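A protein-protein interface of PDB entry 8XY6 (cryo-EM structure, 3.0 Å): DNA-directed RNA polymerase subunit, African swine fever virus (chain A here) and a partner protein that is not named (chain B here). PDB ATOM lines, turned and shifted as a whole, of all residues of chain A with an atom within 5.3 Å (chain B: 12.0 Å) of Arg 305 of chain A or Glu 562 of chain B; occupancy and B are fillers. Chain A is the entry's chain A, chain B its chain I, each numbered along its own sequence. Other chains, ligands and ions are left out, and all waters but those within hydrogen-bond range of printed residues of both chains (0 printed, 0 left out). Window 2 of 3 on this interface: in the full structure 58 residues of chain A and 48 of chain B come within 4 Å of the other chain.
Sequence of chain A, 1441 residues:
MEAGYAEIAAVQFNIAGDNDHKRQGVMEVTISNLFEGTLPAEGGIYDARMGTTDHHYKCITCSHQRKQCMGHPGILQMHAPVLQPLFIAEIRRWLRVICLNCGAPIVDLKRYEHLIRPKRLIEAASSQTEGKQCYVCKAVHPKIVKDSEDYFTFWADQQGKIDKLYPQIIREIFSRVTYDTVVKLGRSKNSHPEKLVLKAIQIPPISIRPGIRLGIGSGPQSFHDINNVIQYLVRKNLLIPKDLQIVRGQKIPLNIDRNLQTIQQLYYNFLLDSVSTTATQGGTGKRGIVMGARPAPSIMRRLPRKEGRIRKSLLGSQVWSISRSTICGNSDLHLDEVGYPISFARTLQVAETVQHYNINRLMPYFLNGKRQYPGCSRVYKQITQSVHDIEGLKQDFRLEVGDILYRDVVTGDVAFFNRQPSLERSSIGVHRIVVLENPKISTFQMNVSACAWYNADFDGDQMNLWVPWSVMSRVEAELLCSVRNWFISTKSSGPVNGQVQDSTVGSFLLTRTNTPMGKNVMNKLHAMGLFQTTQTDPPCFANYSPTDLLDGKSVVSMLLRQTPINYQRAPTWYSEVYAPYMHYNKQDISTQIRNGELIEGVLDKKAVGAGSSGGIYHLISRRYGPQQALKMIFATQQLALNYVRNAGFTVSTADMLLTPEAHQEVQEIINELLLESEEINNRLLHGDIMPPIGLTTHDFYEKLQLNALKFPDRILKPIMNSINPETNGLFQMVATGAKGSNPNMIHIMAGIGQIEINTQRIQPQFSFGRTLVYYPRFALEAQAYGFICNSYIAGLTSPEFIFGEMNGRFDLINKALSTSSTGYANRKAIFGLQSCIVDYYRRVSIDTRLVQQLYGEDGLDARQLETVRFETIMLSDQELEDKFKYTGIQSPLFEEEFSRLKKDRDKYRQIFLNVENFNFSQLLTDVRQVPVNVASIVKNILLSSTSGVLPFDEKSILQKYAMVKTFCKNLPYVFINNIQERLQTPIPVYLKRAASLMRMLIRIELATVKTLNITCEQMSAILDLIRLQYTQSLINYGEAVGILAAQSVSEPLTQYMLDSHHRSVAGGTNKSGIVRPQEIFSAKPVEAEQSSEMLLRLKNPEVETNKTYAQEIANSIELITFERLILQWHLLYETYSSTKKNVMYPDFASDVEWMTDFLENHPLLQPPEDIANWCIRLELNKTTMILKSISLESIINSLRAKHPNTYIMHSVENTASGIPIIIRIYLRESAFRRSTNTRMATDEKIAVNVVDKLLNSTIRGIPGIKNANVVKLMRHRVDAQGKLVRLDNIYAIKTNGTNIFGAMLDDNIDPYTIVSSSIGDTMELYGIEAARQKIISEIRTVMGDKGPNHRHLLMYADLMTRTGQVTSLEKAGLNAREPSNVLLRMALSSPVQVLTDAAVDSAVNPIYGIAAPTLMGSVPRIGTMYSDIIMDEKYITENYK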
ATOM      1  N   ARG A 301      -9.021  12.944 -16.194  1.00  0.00           N
ATOM      2  CA  ARG A 301      -8.051  12.067 -15.547  1.00  0.00           C
ATOM      3  C   ARG A 301      -6.653  12.282 -16.111  1.00  0.00           C
ATOM      4  O   ARG A 301      -5.657  12.031 -15.425  1.00  0.00           O
ATOM      5  CB  ARG A 301      -8.492  10.609 -15.704  1.00  0.00           C
ATOM      6  CG  ARG A 301      -7.490   9.541 -15.273  1.00  0.00           C
ATOM      7  CD  ARG A 301      -6.968   9.753 -13.860  1.00  0.00           C
ATOM      8  NE  ARG A 301      -6.280   8.569 -13.362  1.00  0.00           N
ATOM      9  CZ  ARG A 301      -5.522   8.542 -12.273  1.00  0.00           C
ATOM     10  NH1 ARG A 301      -5.309   9.631 -11.552  1.00  0.00           N
ATOM     11  NH2 ARG A 301      -4.958   7.396 -11.902  1.00  0.00           N
ATOM     12  N   LEU A 303      -5.091  15.040 -16.722  1.00  0.00           N
ATOM     13  CA  LEU A 303      -4.349  16.190 -16.199  1.00  0.00           C
ATOM     14  C   LEU A 303      -3.483  15.838 -14.995  1.00  0.00           C
ATOM     15  O   LEU A 303      -2.251  15.977 -15.077  1.00  0.00           O
ATOM     16  CB  LEU A 303      -5.315  17.325 -15.866  1.00  0.00           C
ATOM     17  CG  LEU A 303      -6.138  18.006 -16.946  1.00  0.00           C
ATOM     18  CD1 LEU A 303      -6.985  19.038 -16.253  1.00  0.00           C
ATOM     19  CD2 LEU A 303      -5.245  18.651 -17.978  1.00  0.00           C
ATOM     20  N   PRO A 304      -4.038  15.385 -13.859  1.00  0.00           N
ATOM     21  CA  PRO A 304      -3.281  15.441 -12.602  1.00  0.00           C
ATOM     22  C   PRO A 304      -2.217  14.368 -12.465  1.00  0.00           C
ATOM     23  O   PRO A 304      -1.947  13.619 -13.407  1.00  0.00           O
ATOM     24  CB  PRO A 304      -4.376  15.264 -11.550  1.00  0.00           C
ATOM     25  CG  PRO A 304      -5.304  14.326 -12.207  1.00  0.00           C
ATOM     26  CD  PRO A 304      -5.342  14.730 -13.655  1.00  0.00           C
ATOM     27  N   ARG A 305      -1.601  14.313 -11.281  1.00  0.00           N
ATOM     28  CA  ARG A 305      -0.565  13.346 -10.928  1.00  0.00           C
ATOM     29  C   ARG A 305       0.718  13.582 -11.716  1.00  0.00           C
ATOM     30  O   ARG A 305       0.736  14.358 -12.676  1.00  0.00           O
ATOM     31  CB  ARG A 305      -1.061  11.912 -11.130  1.00  0.00           C
ATOM     32  CG  ARG A 305      -2.251  11.530 -10.267  1.00  0.00           C
ATOM     33  CD  ARG A 305      -1.840  11.318  -8.819  1.00  0.00           C
ATOM     34  NE  ARG A 305      -2.657  12.106  -7.904  1.00  0.00           N
ATOM     35  CZ  ARG A 305      -2.240  12.575  -6.736  1.00  0.00           C
ATOM     36  NH1 ARG A 305      -1.011  12.354  -6.300  1.00  0.00           N
ATOM     37  NH2 ARG A 305      -3.077  13.287  -5.986  1.00  0.00           N
ATOM     38  N   LYS A 306       1.795  12.910 -11.308  1.00  0.00           N
ATOM     39  CA  LYS A 306       3.107  13.168 -11.893  1.00  0.00           C
ATOM     40  C   LYS A 306       3.135  12.826 -13.376  1.00  0.00           C
ATOM     41  O   LYS A 306       3.698  13.575 -14.182  1.00  0.00           O
ATOM     42  CB  LYS A 306       4.175  12.376 -11.142  1.00  0.00           C
ATOM     43  CG  LYS A 306       5.517  12.323 -11.845  1.00  0.00           C
ATOM     44  CD  LYS A 306       6.591  11.775 -10.928  1.00  0.00           C
ATOM     45  CE  LYS A 306       7.692  11.095 -11.716  1.00  0.00           C
ATOM     46  NZ  LYS A 306       8.234  11.981 -12.780  1.00  0.00           N
ATOM     47  N   GLU A 307       2.539  11.698 -13.757  1.00  0.00           N
ATOM     48  CA  GLU A 307       2.543  11.245 -15.139  1.00  0.00           C
ATOM     49  C   GLU A 307       1.361  11.782 -15.936  1.00  0.00           C
ATOM     50  O   GLU A 307       1.047  11.246 -17.003  1.00  0.00           O
ATOM     51  CB  GLU A 307       2.568   9.715 -15.194  1.00  0.00           C
ATOM     52  CG  GLU A 307       1.280   9.030 -14.756  1.00  0.00           C
ATOM     53  CD  GLU A 307       0.986   9.207 -13.282  1.00  0.00           C
ATOM     54  OE1 GLU A 307       1.929   9.106 -12.470  1.00  0.00           O
ATOM     55  OE2 GLU A 307      -0.189   9.443 -12.936  1.00  0.00           O
ATOM     56  N   GLY A 308       0.708  12.829 -15.447  1.00  0.00           N
ATOM     57  CA  GLY A 308      -0.415  13.419 -16.136  1.00  0.00           C
ATOM     58  C   GLY A 308       0.028  14.379 -17.219  1.00  0.00           C
ATOM     59  O   GLY A 308       1.194  14.448 -17.602  1.00  0.00           O
ATOM     60  N   ARG A 311       2.324  17.833 -15.416  1.00  0.00           N
ATOM     61  CA  ARG A 311       3.648  17.661 -14.830  1.00  0.00           C
ATOM     62  C   ARG A 311       4.557  16.799 -15.694  1.00  0.00           C
ATOM     63  O   ARG A 311       5.770  16.767 -15.466  1.00  0.00           O
ATOM     64  CB  ARG A 311       3.518  17.067 -13.429  1.00  0.00           C
ATOM     65  CG  ARG A 311       2.875  18.014 -12.432  1.00  0.00           C
ATOM     66  CD  ARG A 311       2.725  17.374 -11.066  1.00  0.00           C
ATOM     67  NE  ARG A 311       3.996  16.885 -10.550  1.00  0.00           N
ATOM     68  CZ  ARG A 311       4.127  16.166  -9.444  1.00  0.00           C
ATOM     69  NH1 ARG A 311       3.080  15.841  -8.705  1.00  0.00           N
ATOM     70  NH2 ARG A 311       5.337  15.762  -9.073  1.00  0.00           N
ATOM     71  N   TYR A 824       8.564  16.487  -1.812  1.00  0.00           N
ATOM     72  CA  TYR A 824       7.361  17.309  -1.720  1.00  0.00           C
ATOM     73  C   TYR A 824       7.665  18.673  -1.125  1.00  0.00           C
ATOM     74  O   TYR A 824       7.093  19.684  -1.557  1.00  0.00           O
ATOM     75  CB  TYR A 824       6.271  16.614  -0.896  1.00  0.00           C
ATOM     76  CG  TYR A 824       6.092  15.130  -1.128  1.00  0.00           C
ATOM     77  CD1 TYR A 824       6.967  14.204  -0.584  1.00  0.00           C
ATOM     78  CD2 TYR A 824       5.005  14.652  -1.851  1.00  0.00           C
ATOM     79  CE1 TYR A 824       6.791  12.850  -0.785  1.00  0.00           C
ATOM     80  CE2 TYR A 824       4.821  13.301  -2.056  1.00  0.00           C
ATOM     81  CZ  TYR A 824       5.717  12.405  -1.519  1.00  0.00           C
ATOM     82  OH  TYR A 824       5.542  11.055  -1.717  1.00  0.00           O
ATOM     83  N   ASP B 553      -6.995   6.049   4.688  1.00  0.00           N
ATOM     84  CA  ASP B 553      -6.704   7.477   4.662  1.00  0.00           C
ATOM     85  C   ASP B 553      -5.867   7.742   3.424  1.00  0.00           C
ATOM     86  O   ASP B 553      -4.885   7.037   3.174  1.00  0.00           O
ATOM     87  CB  ASP B 553      -5.971   7.931   5.929  1.00  0.00           C
ATOM     88  CG  ASP B 553      -5.529   9.380   5.860  1.00  0.00           C
ATOM     89  OD1 ASP B 553      -6.332  10.227   5.415  1.00  0.00           O
ATOM     90  OD2 ASP B 553      -4.380   9.673   6.249  1.00  0.00           O
ATOM     91  N   ARG B 554      -6.262   8.742   2.644  1.00  0.00           N
ATOM     92  CA  ARG B 554      -5.616   9.028   1.365  1.00  0.00           C
ATOM     93  C   ARG B 554      -4.478  10.007   1.611  1.00  0.00           C
ATOM     94  O   ARG B 554      -4.663  11.224   1.632  1.00  0.00           O
ATOM     95  CB  ARG B 554      -6.628   9.567   0.362  1.00  0.00           C
ATOM     96  CG  ARG B 554      -7.722   8.569   0.001  1.00  0.00           C
ATOM     97  CD  ARG B 554      -8.904   8.648   0.961  1.00  0.00           C
ATOM     98  NE  ARG B 554     -10.120   8.064   0.408  1.00  0.00           N
ATOM     99  CZ  ARG B 554     -10.817   8.580  -0.595  1.00  0.00           C
ATOM    100  NH1 ARG B 554     -10.449   9.704  -1.187  1.00  0.00           N
ATOM    101  NH2 ARG B 554     -11.914   7.955  -1.013  1.00  0.00           N
ATOM    102  N   LEU B 555      -3.280   9.463   1.806  1.00  0.00           N
ATOM    103  CA  LEU B 555      -2.100  10.266   2.079  1.00  0.00           C
ATOM    104  C   LEU B 555      -0.939   9.752   1.244  1.00  0.00           C
ATOM    105  O   LEU B 555      -0.913   8.594   0.820  1.00  0.00           O
ATOM    106  CB  LEU B 555      -1.737  10.245   3.570  1.00  0.00           C
ATOM    107  CG  LEU B 555      -1.293  11.576   4.181  1.00  0.00           C
ATOM    108  CD1 LEU B 555      -2.011  12.744   3.516  1.00  0.00           C
ATOM    109  CD2 LEU B 555      -1.537  11.576   5.682  1.00  0.00           C
ATOM    110  N   ASP B 556       0.025  10.638   1.006  1.00  0.00           N
ATOM    111  CA  ASP B 556       1.195  10.277   0.221  1.00  0.00           C
ATOM    112  C   ASP B 556       2.040   9.253   0.963  1.00  0.00           C
ATOM    113  O   ASP B 556       2.243   9.357   2.176  1.00  0.00           O
ATOM    114  CB  ASP B 556       2.025  11.521  -0.090  1.00  0.00           C
ATOM    115  CG  ASP B 556       1.194  12.641  -0.678  1.00  0.00           C
ATOM    116  OD1 ASP B 556       0.144  12.345  -1.285  1.00  0.00           O
ATOM    117  OD2 ASP B 556       1.590  13.816  -0.534  1.00  0.00           O
ATOM    118  N   ASP B 557       2.525   8.261   0.230  1.00  0.00           N
ATOM    119  CA  ASP B 557       3.427   7.272   0.796  1.00  0.00           C
ATOM    120  C   ASP B 557       4.728   7.960   1.191  1.00  0.00           C
ATOM    121  O   ASP B 557       5.363   8.601   0.339  1.00  0.00           O
ATOM    122  CB  ASP B 557       3.678   6.158  -0.218  1.00  0.00           C
ATOM    123  CG  ASP B 557       4.968   5.403   0.039  1.00  0.00           C
ATOM    124  OD1 ASP B 557       5.238   5.042   1.203  1.00  0.00           O
ATOM    125  OD2 ASP B 557       5.710   5.162  -0.937  1.00  0.00           O
ATOM    126  N   PRO B 558       5.161   7.863   2.452  1.00  0.00           N
ATOM    127  CA  PRO B 558       6.337   8.625   2.896  1.00  0.00           C
ATOM    128  C   PRO B 558       7.638   8.188   2.250  1.00  0.00           C
ATOM    129  O   PRO B 558       8.664   8.835   2.477  1.00  0.00           O
ATOM    130  CB  PRO B 558       6.361   8.377   4.410  1.00  0.00           C
ATOM    131  CG  PRO B 558       5.669   7.081   4.588  1.00  0.00           C
ATOM    132  CD  PRO B 558       4.614   7.014   3.522  1.00  0.00           C
ATOM    133  N   PHE B 559       7.633   7.107   1.474  1.00  0.00           N
ATOM    134  CA  PHE B 559       8.786   6.688   0.693  1.00  0.00           C
ATOM    135  C   PHE B 559       8.610   6.937  -0.798  1.00  0.00           C
ATOM    136  O   PHE B 559       9.524   6.640  -1.573  1.00  0.00           O
ATOM    137  CB  PHE B 559       9.064   5.200   0.917  1.00  0.00           C
ATOM    138  CG  PHE B 559       9.652   4.881   2.253  1.00  0.00           C
ATOM    139  CD1 PHE B 559       8.838   4.618   3.334  1.00  0.00           C
ATOM    140  CD2 PHE B 559      11.022   4.801   2.418  1.00  0.00           C
ATOM    141  CE1 PHE B 559       9.379   4.311   4.562  1.00  0.00           C
ATOM    142  CE2 PHE B 559      11.566   4.487   3.641  1.00  0.00           C
ATOM    143  CZ  PHE B 559      10.744   4.239   4.713  1.00  0.00           C
ATOM    144  N   SER B 560       7.464   7.466  -1.218  1.00  0.00           N
ATOM    145  CA  SER B 560       7.171   7.588  -2.639  1.00  0.00           C
ATOM    146  C   SER B 560       7.974   8.719  -3.263  1.00  0.00           C
ATOM    147  O   SER B 560       7.955   9.853  -2.775  1.00  0.00           O
ATOM    148  CB  SER B 560       5.678   7.827  -2.851  1.00  0.00           C
ATOM    149  OG  SER B 560       5.216   8.893  -2.041  1.00  0.00           O
ATOM    150  N   ILE B 561       8.679   8.408  -4.347  1.00  0.00           N
ATOM    151  CA  ILE B 561       9.401   9.432  -5.119  1.00  0.00           C
ATOM    152  C   ILE B 561       8.412   9.934  -6.165  1.00  0.00           C
ATOM    153  O   ILE B 561       8.400   9.515  -7.324  1.00  0.00           O
ATOM    154  CB  ILE B 561      10.692   8.888  -5.736  1.00  0.00           C
ATOM    155  CG1 ILE B 561      11.358   7.890  -4.790  1.00  0.00           C
ATOM    156  CG2 ILE B 561      11.642  10.022  -6.060  1.00  0.00           C
ATOM    157  CD1 ILE B 561      11.926   8.516  -3.540  1.00  0.00           C
ATOM    158  N   GLU B 562       7.560  10.862  -5.743  1.00  0.00           N
ATOM    159  CA  GLU B 562       6.486  11.375  -6.585  1.00  0.00           C
ATOM    160  C   GLU B 562       6.644  12.842  -6.938  1.00  0.00           C
ATOM    161  O   GLU B 562       6.392  13.224  -8.082  1.00  0.00           O
ATOM    162  CB  GLU B 562       5.132  11.152  -5.898  1.00  0.00           C
ATOM    163  CG  GLU B 562       4.087  12.219  -6.175  1.00  0.00           C
ATOM    164  CD  GLU B 562       2.880  12.092  -5.268  1.00  0.00           C
ATOM    165  OE1 GLU B 562       2.756  11.051  -4.589  1.00  0.00           O
ATOM    166  OE2 GLU B 562       2.057  13.030  -5.234  1.00  0.00           O
ATOM    167  N   ASP B 563       7.059  13.683  -5.993  1.00  0.00           N
ATOM    168  CA  ASP B 563       7.325  15.082  -6.289  1.00  0.00           C
ATOM    169  C   ASP B 563       8.766  15.340  -6.705  1.00  0.00           C
ATOM    170  O   ASP B 563       9.085  16.465  -7.106  1.00  0.00           O
ATOM    171  CB  ASP B 563       6.970  15.959  -5.085  1.00  0.00           C
ATOM    172  CG  ASP B 563       5.483  16.237  -4.989  1.00  0.00           C
ATOM    173  OD1 ASP B 563       4.732  15.729  -5.848  1.00  0.00           O
ATOM    174  OD2 ASP B 563       5.066  16.966  -4.065  1.00  0.00           O
ATOM    175  N   VAL B 564       9.637  14.340  -6.623  1.00  0.00           N
ATOM    176  CA  VAL B 564      10.976  14.425  -7.194  1.00  0.00           C
ATOM    177  C   VAL B 564      10.909  13.860  -8.606  1.00  0.00           C
ATOM    178  O   VAL B 564      10.416  12.747  -8.817  1.00  0.00           O
ATOM    179  CB  VAL B 564      12.004  13.667  -6.341  1.00  0.00           C
ATOM    180  CG1 VAL B 564      13.140  13.174  -7.203  1.00  0.00           C
ATOM    181  CG2 VAL B 564      12.556  14.562  -5.259  1.00  0.00           C
ATOM    182  N   ASP B 565      11.389  14.634  -9.579  1.00  0.00           N
ATOM    183  CA  ASP B 565      11.300  14.249 -10.986  1.00  0.00           C
ATOM    184  C   ASP B 565      12.642  13.667 -11.418  1.00  0.00           C
ATOM    185  O   ASP B 565      13.533  14.359 -11.914  1.00  0.00           O
ATOM    186  CB  ASP B 565      10.889  15.442 -11.837  1.00  0.00           C
ATOM    187  CG  ASP B 565      10.025  15.046 -13.012  1.00  0.00           C
ATOM    188  OD1 ASP B 565       9.483  13.923 -12.997  1.00  0.00           O
ATOM    189  OD2 ASP B 565       9.872  15.863 -13.943  1.00  0.00           O
ATOM    190  N   ILE B 566      12.778  12.357 -11.223  1.00  0.00           N
ATOM    191  CA  ILE B 566      13.993  11.623 -11.557  1.00  0.00           C
ATOM    192  C   ILE B 566      13.603  10.392 -12.366  1.00  0.00           C
ATOM    193  O   ILE B 566      12.618   9.716 -12.048  1.00  0.00           O
ATOM    194  CB  ILE B 566      14.780  11.235 -10.288  1.00  0.00           C
ATOM    195  CG1 ILE B 566      15.988  10.368 -10.635  1.00  0.00           C
ATOM    196  CG2 ILE B 566      13.883  10.511  -9.310  1.00  0.00           C
ATOM    197  CD1 ILE B 566      17.087  10.433  -9.607  1.00  0.00           C
ATOM    198  N   SER B 567      14.363  10.113 -13.421  1.00  0.00           N
ATOM    199  CA  SER B 567      14.020   9.027 -14.326  1.00  0.00           C
ATOM    200  C   SER B 567      14.312   7.672 -13.684  1.00  0.00           C
ATOM    201  O   SER B 567      15.009   7.566 -12.673  1.00  0.00           O
ATOM    202  CB  SER B 567      14.775   9.168 -15.646  1.00  0.00           C
ATOM    203  OG  SER B 567      14.472   8.099 -16.524  1.00  0.00           O
ATOM    204  N   LEU B 568      13.760   6.621 -14.298  1.00  0.00           N
ATOM    205  CA  LEU B 568      13.860   5.277 -13.736  1.00  0.00           C
ATOM    206  C   LEU B 568      15.306   4.797 -13.673  1.00  0.00           C
ATOM    207  O   LEU B 568      15.733   4.226 -12.663  1.00  0.00           O
ATOM    208  CB  LEU B 568      13.009   4.311 -14.564  1.00  0.00           C
ATOM    209  CG  LEU B 568      12.974   2.808 -14.254  1.00  0.00           C
ATOM    210  CD1 LEU B 568      13.030   2.509 -12.763  1.00  0.00           C
ATOM    211  CD2 LEU B 568      11.743   2.171 -14.880  1.00  0.00           C
ATOM    212  N   LEU B 571      17.658   6.465 -11.026  1.00  0.00           N
ATOM    213  CA  LEU B 571      17.361   6.309  -9.606  1.00  0.00           C
ATOM    214  C   LEU B 571      18.535   5.719  -8.840  1.00  0.00           C
ATOM    215  O   LEU B 571      18.544   5.771  -7.605  1.00  0.00           O
ATOM    216  CB  LEU B 571      16.122   5.438  -9.397  1.00  0.00           C
ATOM    217  CG  LEU B 571      14.799   5.946  -9.968  1.00  0.00           C
ATOM    218  CD1 LEU B 571      13.826   4.808 -10.161  1.00  0.00           C
ATOM    219  CD2 LEU B 571      14.206   6.987  -9.050  1.00  0.00           C
ATOM    220  N   LEU B 574      20.386   8.027  -6.376  1.00  0.00           N
ATOM    221  CA  LEU B 574      19.915   8.107  -5.002  1.00  0.00           C
ATOM    222  C   LEU B 574      20.542   7.052  -4.102  1.00  0.00           C
ATOM    223  O   LEU B 574      20.375   7.130  -2.882  1.00  0.00           O
ATOM    224  CB  LEU B 574      18.393   7.970  -4.972  1.00  0.00           C
ATOM    225  CG  LEU B 574      17.572   9.253  -4.865  1.00  0.00           C
ATOM    226  CD1 LEU B 574      18.099  10.311  -5.811  1.00  0.00           C
ATOM    227  CD2 LEU B 574      16.119   8.955  -5.171  1.00  0.00           C
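The guanidinium group (NH1) of Arg 305 of chain A lies within salt-bridge range of the side-chain carboxylate (OE2) of Glu 562 of chain B, 3.3 Å away. The guanidinium group of Arg 311 of chain A is in hydrogen-bond range of the backbone carbonyl oxygen of Glu 562 of chain B, 2.9 Å away. NH2 of Arg 311 of chain A lies within salt-bridge range of OD1 of Asp 563 of chain B (3.3 Å). The side-chain hydroxyl (OH) of Tyr 824 of chain A is in hydrogen-bond range of the backbone carbonyl oxygen (O) of Asp 557 of chain B, at 3.2 Å. OH of Tyr 824 of chain A is in hydrogen-bond range of O of Ser 560 of chain B, at 2.9 Å. The side-chain amino group (NZ) of Lys 306 of chain A sits close to the side-chain carboxylate (OD1) of Asp 565 of chain B, 2.3 Å away.
O of Glu 562 of chain B touches CD of Lys 306 of chain A, 3.2 Å away. OD2 of Asp 556 of chain B touches CE2 of Tyr 824 of chain A, 3.6 Å away. Tyr 824 of chain A touches Glu 562 of chain B. Tyr 824 of chain A touches Asp 563 of chain B.
Of the 9 printed residues of chain A, 4 touch a printed residue of chain B. Hydrophobic or aromatic side chains of chain A within 4 Å of the printed part of chain B: Tyr 824. Along chain A the printed residues that touch a printed residue of chain B span positions 305 to 824. Along chain B the printed residues that touch a printed residue of chain A span positions 556 to 565. Among the printed residues, Asp or Glu carboxylates within 4 Å of a Lys or Arg side-chain nitrogen of the other chain: Arg 305 of chain A with Glu 562 of chain B (3.3 Å), Lys 306 of chain A with Asp 565 of chain B (2.3 Å) and Arg 311 of chain A with Asp 563 of chain B (3.3 Å).
Of chain B, only Glu 562 comes within 4 Å of Arg 305 of chain A. Glu 562 of chain B touches just these residues of chain A: Arg 305 (3.3 Å), Lys 306 (3.2 Å), Arg 311 (2.9 Å) and Tyr 824 (3.9 Å). Of chain B, only Glu 562 and Asp 565 come within 4 Å of Lys 306 of chain A. Gly 308 of chain A touches none of the printed residues of chain B. Arg 311 of chain A touches just these residues of chain B: Glu 562 (2.9 Å) and Asp 563 (3.3 Å). Of the printed residues of chain A, Asp 557 of chain B touches Tyr 824. Printed residues of chain A within 4 Å of Ser 560 of chain B: Tyr 824. Of the printed residues of chain A, Asp 565 of chain B touches Lys 306. Leu 568 of chain B touches none of the printed residues of chain A. The nearest residue of chain B that does not touch Arg 305 of chain A is Asp 556 of chain B (5.1 Å). The nearest printed residue of chain A that does not touch Glu 562 of chain B is Glu 307 of chain A (7.0 Å).
The backbone NH of Phe 559 of chain B sits close to the side-chain carboxylate of Asp 557 of chain B (3.2 Å). O of Asp 557 of chain B sits at hydrogen-bond distance from OG of Ser 560 of chain B.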
